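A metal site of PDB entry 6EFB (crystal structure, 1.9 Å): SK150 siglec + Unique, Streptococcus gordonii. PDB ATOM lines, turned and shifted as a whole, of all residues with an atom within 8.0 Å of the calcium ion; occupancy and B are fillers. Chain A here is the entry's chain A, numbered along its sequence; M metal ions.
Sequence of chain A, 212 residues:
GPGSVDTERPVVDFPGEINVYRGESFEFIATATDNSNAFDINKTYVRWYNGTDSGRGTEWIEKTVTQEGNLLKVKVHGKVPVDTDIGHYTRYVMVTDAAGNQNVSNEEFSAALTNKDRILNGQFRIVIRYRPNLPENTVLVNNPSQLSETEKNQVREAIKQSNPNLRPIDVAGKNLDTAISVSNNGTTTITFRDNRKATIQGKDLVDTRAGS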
ATOM      1  N   ASP A   6     -20.653   3.912  16.433  1.00  0.00           N
ATOM      2  CA  ASP A   6     -20.678   2.452  16.573  1.00  0.00           C
ATOM      3  C   ASP A   6     -20.222   2.017  17.975  1.00  0.00           C
ATOM      4  O   ASP A   6     -19.043   2.104  18.305  1.00  0.00           O
ATOM      5  CB  ASP A   6     -19.807   1.805  15.498  1.00  0.00           C
ATOM      6  CG  ASP A   6     -19.882   0.288  15.503  1.00  0.00           C
ATOM      7  OD1 ASP A   6     -20.669  -0.273  16.306  1.00  0.00           O
ATOM      8  OD2 ASP A   6     -19.153  -0.338  14.702  1.00  0.00           O
ATOM      9  N   THR A   7     -21.180   1.545  18.781  1.00  0.00           N
ATOM     10  CA  THR A   7     -20.896   1.019  20.116  1.00  0.00           C
ATOM     11  C   THR A   7     -21.377  -0.418  20.277  1.00  0.00           C
ATOM     12  O   THR A   7     -21.541  -0.884  21.404  1.00  0.00           O
ATOM     13  CB  THR A   7     -21.534   1.902  21.195  1.00  0.00           C
ATOM     14  N   GLU A   8     -21.603  -1.126  19.173  1.00  0.00           N
ATOM     15  CA  GLU A   8     -21.987  -2.527  19.195  1.00  0.00           C
ATOM     16  C   GLU A   8     -20.746  -3.375  18.880  1.00  0.00           C
ATOM     17  O   GLU A   8     -20.051  -3.114  17.899  1.00  0.00           O
ATOM     18  CB  GLU A   8     -23.098  -2.811  18.185  1.00  0.00           C
ATOM     19  CG  GLU A   8     -23.481  -4.269  18.033  1.00  0.00           C
ATOM     20  CD  GLU A   8     -24.559  -4.474  16.990  1.00  0.00           C
ATOM     21  OE1 GLU A   8     -25.359  -3.538  16.767  1.00  0.00           O
ATOM     22  OE2 GLU A   8     -24.617  -5.572  16.377  1.00  0.00           O
ATOM     23  N   ARG A   9     -20.475  -4.374  19.729  1.00  0.00           N
ATOM     24  CA  ARG A   9     -19.285  -5.202  19.600  1.00  0.00           C
ATOM     25  C   ARG A   9     -19.433  -6.191  18.453  1.00  0.00           C
ATOM     26  O   ARG A   9     -20.524  -6.713  18.212  1.00  0.00           O
ATOM     27  CB  ARG A   9     -19.007  -5.955  20.900  1.00  0.00           C
ATOM     28  CG  ARG A   9     -18.612  -5.080  22.101  1.00  0.00           C
ATOM     29  CD  ARG A   9     -18.303  -5.921  23.348  1.00  0.00           C
ATOM     30  NE  ARG A   9     -18.106  -5.119  24.559  1.00  0.00           N
ATOM     31  CZ  ARG A   9     -16.952  -4.550  24.908  1.00  0.00           C
ATOM     32  NH1 ARG A   9     -15.884  -4.667  24.135  1.00  0.00           N
ATOM     33  NH2 ARG A   9     -16.878  -3.830  26.032  1.00  0.00           N
ATOM     34  N   PRO A  10     -18.357  -6.472  17.728  1.00  0.00           N
ATOM     35  CA  PRO A  10     -18.380  -7.573  16.751  1.00  0.00           C
ATOM     36  C   PRO A  10     -18.540  -8.900  17.482  1.00  0.00           C
ATOM     37  O   PRO A  10     -18.405  -9.005  18.705  1.00  0.00           O
ATOM     38  CB  PRO A  10     -17.031  -7.458  16.047  1.00  0.00           C
ATOM     39  CG  PRO A  10     -16.132  -6.853  17.073  1.00  0.00           C
ATOM     40  CD  PRO A  10     -17.002  -5.902  17.865  1.00  0.00           C
ATOM     41  N   VAL A  11     -18.884  -9.941  16.716  1.00  0.00           N
ATOM     42  CA  VAL A  11     -19.231 -11.247  17.267  1.00  0.00           C
ATOM     43  C   VAL A  11     -18.525 -12.334  16.476  1.00  0.00           C
ATOM     44  O   VAL A  11     -18.693 -12.430  15.259  1.00  0.00           O
ATOM     45  CB  VAL A  11     -20.753 -11.487  17.261  1.00  0.00           C
ATOM     46  CG1 VAL A  11     -21.089 -12.731  18.052  1.00  0.00           C
ATOM     47  CG2 VAL A  11     -21.484 -10.277  17.831  1.00  0.00           C
ATOM     48  N   THR A  33     -18.834 -11.155  12.510  1.00  0.00           N
ATOM     49  CA  THR A  33     -19.755 -10.202  11.939  1.00  0.00           C
ATOM     50  C   THR A  33     -19.762  -8.946  12.802  1.00  0.00           C
ATOM     51  O   THR A  33     -19.378  -8.980  13.976  1.00  0.00           O
ATOM     52  CB  THR A  33     -21.168 -10.779  11.853  1.00  0.00           C
ATOM     53  OG1 THR A  33     -21.615 -11.149  13.166  1.00  0.00           O
ATOM     54  CG2 THR A  33     -21.181 -12.014  10.977  1.00  0.00           C
ATOM     55  N   ASP A  34     -20.187  -7.836  12.205  1.00  0.00           N
ATOM     56  CA  ASP A  34     -20.325  -6.590  12.944  1.00  0.00           C
ATOM     57  C   ASP A  34     -21.356  -5.701  12.267  1.00  0.00           C
ATOM     58  O   ASP A  34     -21.468  -5.688  11.036  1.00  0.00           O
ATOM     59  CB  ASP A  34     -18.998  -5.854  13.075  1.00  0.00           C
ATOM     60  CG  ASP A  34     -19.077  -4.681  14.015  1.00  0.00           C
ATOM     61  OD1 ASP A  34     -19.224  -4.923  15.235  1.00  0.00           O
ATOM     62  OD2 ASP A  34     -19.045  -3.524  13.531  1.00  0.00           O
ATOM     63  N   ASN A  35     -22.089  -4.943  13.093  1.00  0.00           N
ATOM     64  CA  ASN A  35     -23.139  -4.066  12.587  1.00  0.00           C
ATOM     65  C   ASN A  35     -22.622  -3.089  11.546  1.00  0.00           C
ATOM     66  O   ASN A  35     -23.348  -2.723  10.614  1.00  0.00           O
ATOM     67  CB  ASN A  35     -23.772  -3.299  13.757  1.00  0.00           C
ATOM     68  CG  ASN A  35     -22.760  -2.457  14.514  1.00  0.00           C
ATOM     69  OD1 ASN A  35     -21.774  -2.982  15.029  1.00  0.00           O
ATOM     70  ND2 ASN A  35     -22.985  -1.159  14.567  1.00  0.00           N
ATOM     71  N   SER A  36     -21.370  -2.647  11.677  1.00  0.00           N
ATOM     72  CA  SER A  36     -20.753  -1.729  10.723  1.00  0.00           C
ATOM     73  C   SER A  36     -20.170  -2.424   9.500  1.00  0.00           C
ATOM     74  O   SER A  36     -19.791  -1.731   8.547  1.00  0.00           O
ATOM     75  CB  SER A  36     -19.660  -0.915  11.414  1.00  0.00           C
ATOM     76  OG  SER A  36     -18.521  -1.723  11.672  1.00  0.00           O
ATOM     77  N   ASN A  37     -20.045  -3.759   9.520  1.00  0.00           N
ATOM     78  CA  ASN A  37     -19.445  -4.537   8.441  1.00  0.00           C
ATOM     79  C   ASN A  37     -17.998  -4.134   8.157  1.00  0.00           C
ATOM     80  O   ASN A  37     -17.451  -4.446   7.090  1.00  0.00           O
ATOM     81  CB  ASN A  37     -20.270  -4.450   7.152  1.00  0.00           C
ATOM     82  CG  ASN A  37     -21.645  -5.008   7.320  1.00  0.00           C
ATOM     83  OD1 ASN A  37     -21.858  -5.951   8.091  1.00  0.00           O
ATOM     84  ND2 ASN A  37     -22.609  -4.457   6.592  1.00  0.00           N
ATOM     85  N   ALA A  38     -17.363  -3.434   9.081  1.00  0.00           N
ATOM     86  CA  ALA A  38     -16.008  -2.969   8.890  1.00  0.00           C
ATOM     87  C   ALA A  38     -15.182  -3.365  10.095  1.00  0.00           C
ATOM     88  O   ALA A  38     -15.664  -3.310  11.240  1.00  0.00           O
ATOM     89  CB  ALA A  38     -15.963  -1.454   8.680  1.00  0.00           C
ATOM     90  N   PHE A  39     -13.950  -3.798   9.845  1.00  0.00           N
ATOM     91  CA  PHE A  39     -13.078  -4.316  10.881  1.00  0.00           C
ATOM     92  C   PHE A  39     -11.719  -3.639  10.810  1.00  0.00           C
ATOM     93  O   PHE A  39     -11.273  -3.203   9.756  1.00  0.00           O
ATOM     94  CB  PHE A  39     -12.894  -5.834  10.762  1.00  0.00           C
ATOM     95  CG  PHE A  39     -14.158  -6.603  10.969  1.00  0.00           C
ATOM     96  CD1 PHE A  39     -15.015  -6.861   9.912  1.00  0.00           C
ATOM     97  CD2 PHE A  39     -14.498  -7.067  12.229  1.00  0.00           C
ATOM     98  CE1 PHE A  39     -16.193  -7.580  10.105  1.00  0.00           C
ATOM     99  CE2 PHE A  39     -15.654  -7.783  12.434  1.00  0.00           C
ATOM    100  CZ  PHE A  39     -16.514  -8.037  11.364  1.00  0.00           C
ATOM    101  N   THR A  96     -11.623  -6.829  16.261  1.00  0.00           N
ATOM    102  CA  THR A  96     -11.907  -5.423  16.534  1.00  0.00           C
ATOM    103  C   THR A  96     -12.591  -4.804  15.327  1.00  0.00           C
ATOM    104  O   THR A  96     -12.060  -4.875  14.207  1.00  0.00           O
ATOM    105  CB  THR A  96     -10.629  -4.647  16.842  1.00  0.00           C
ATOM    106  OG1 THR A  96      -9.889  -5.332  17.864  1.00  0.00           O
ATOM    107  CG2 THR A  96     -10.966  -3.246  17.301  1.00  0.00           C
ATOM    108  N   ASP A  97     -13.747  -4.178  15.525  1.00  0.00           N
ATOM    109  CA  ASP A  97     -14.387  -3.485  14.422  1.00  0.00           C
ATOM    110  C   ASP A  97     -13.612  -2.213  14.076  1.00  0.00           C
ATOM    111  O   ASP A  97     -12.649  -1.833  14.750  1.00  0.00           O
ATOM    112  CB  ASP A  97     -15.864  -3.190  14.730  1.00  0.00           C
ATOM    113  CG  ASP A  97     -16.061  -2.298  15.949  1.00  0.00           C
ATOM    114  OD1 ASP A  97     -15.173  -1.497  16.297  1.00  0.00           O
ATOM    115  OD2 ASP A  97     -17.146  -2.387  16.574  1.00  0.00           O
ATOM    116  N   ALA A  98     -14.052  -1.538  13.018  1.00  0.00           N
ATOM    117  CA  ALA A  98     -13.370  -0.315  12.582  1.00  0.00           C
ATOM    118  C   ALA A  98     -13.459   0.783  13.636  1.00  0.00           C
ATOM    119  O   ALA A  98     -12.562   1.638  13.722  1.00  0.00           O
ATOM    120  CB  ALA A  98     -13.949   0.176  11.261  1.00  0.00           C
ATOM    121  N   ALA A  99     -14.511   0.777  14.459  1.00  0.00           N
ATOM    122  CA  ALA A  99     -14.671   1.778  15.495  1.00  0.00           C
ATOM    123  C   ALA A  99     -13.887   1.448  16.764  1.00  0.00           C
ATOM    124  O   ALA A  99     -13.999   2.190  17.754  1.00  0.00           O
ATOM    125  CB  ALA A  99     -16.165   1.948  15.829  1.00  0.00           C
ATOM    126  N   GLY A 100     -13.111   0.369  16.762  1.00  0.00           N
ATOM    127  CA  GLY A 100     -12.253   0.051  17.889  1.00  0.00           C
ATOM    128  C   GLY A 100     -12.867  -0.832  18.950  1.00  0.00           C
ATOM    129  O   GLY A 100     -12.224  -1.072  19.977  1.00  0.00           O
ATOM    130  N   ASN A 101     -14.096  -1.318  18.742  1.00  0.00           N
ATOM    131  CA  ASN A 101     -14.737  -2.197  19.720  1.00  0.00           C
ATOM    132  C   ASN A 101     -14.278  -3.634  19.506  1.00  0.00           C
ATOM    133  O   ASN A 101     -14.381  -4.184  18.407  1.00  0.00           O
ATOM    134  CB  ASN A 101     -16.262  -2.125  19.582  1.00  0.00           C
ATOM    135  CG  ASN A 101     -16.768  -0.701  19.426  1.00  0.00           C
ATOM    136  OD1 ASN A 101     -16.336   0.206  20.146  1.00  0.00           O
ATOM    137  ND2 ASN A 101     -17.673  -0.490  18.470  1.00  0.00           N
ATOM    138  N   GLN A 102     -13.757  -4.237  20.573  1.00  0.00           N
ATOM    139  CA  GLN A 102     -13.363  -5.641  20.559  1.00  0.00           C
ATOM    140  C   GLN A 102     -14.569  -6.532  20.833  1.00  0.00           C
ATOM    141  O   GLN A 102     -15.556  -6.105  21.452  1.00  0.00           O
ATOM    142  CB  GLN A 102     -12.266  -5.900  21.597  1.00  0.00           C
ATOM    143  CG  GLN A 102     -10.995  -5.128  21.323  1.00  0.00           C
ATOM    144  CD  GLN A 102     -10.055  -5.078  22.514  1.00  0.00           C
ATOM    145  OE1 GLN A 102     -10.324  -5.650  23.567  1.00  0.00           O
ATOM    146  NE2 GLN A 102      -8.933  -4.379  22.347  1.00  0.00           N
HETATM  147 CA    CA M   1     -19.535  -2.469  15.776  1.00  0.00          CA
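ND2 of Asn 101 is in hydrogen-bond range of O of Asp 6 (2.9 Å).
OG of Ser 36 sits close to OD2 of Asp 6, 3.4 Å away.
The side-chain carboxylate of Asp 97 sits at hydrogen-bond distance from the backbone NH of Asn 101, at 2.7 Å.
The side-chain carboxylate of Asp 97 is in hydrogen-bond range of the backbone NH of Ala 99 (3.0 Å).
The side-chain carboxylate of Asp 97 lies within hydrogen-bond range of the backbone NH of Gly 100.
OD2 of Asp 34 sits close to OG of Ser 36.
OD1 of Asn 37 lies close to O of Asp 34 (3.0 Å).
Asn 101 touches the calcium ion.
Within 4 Å of the calcium ion: Asp 6, Glu 8, Asp 34, Asn 35, Asp 97 and Asn 101.
The nearest printed residue that does not touch the calcium ion is Ser 36 (4.3 Å).
The calcium ion is bound by O of Glu 8.
OD1 of Asn 35 binds the calcium ion (2.4 Å).
The side-chain carboxylate (OD2) of Asp 6 is bound to the calcium ion, 2.4 Å away.
OD2 of Asp 97 is bound to the calcium ion, 2.5 Å away.
The calcium ion is bound by OD1 of Asp 6, 2.5 Å away.
The side-chain carboxylate (OD2) of Asp 34 binds the calcium ion, at 2.5 Å.
OD1 of Asp 34 is bound to the calcium ion (2.5 Å).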
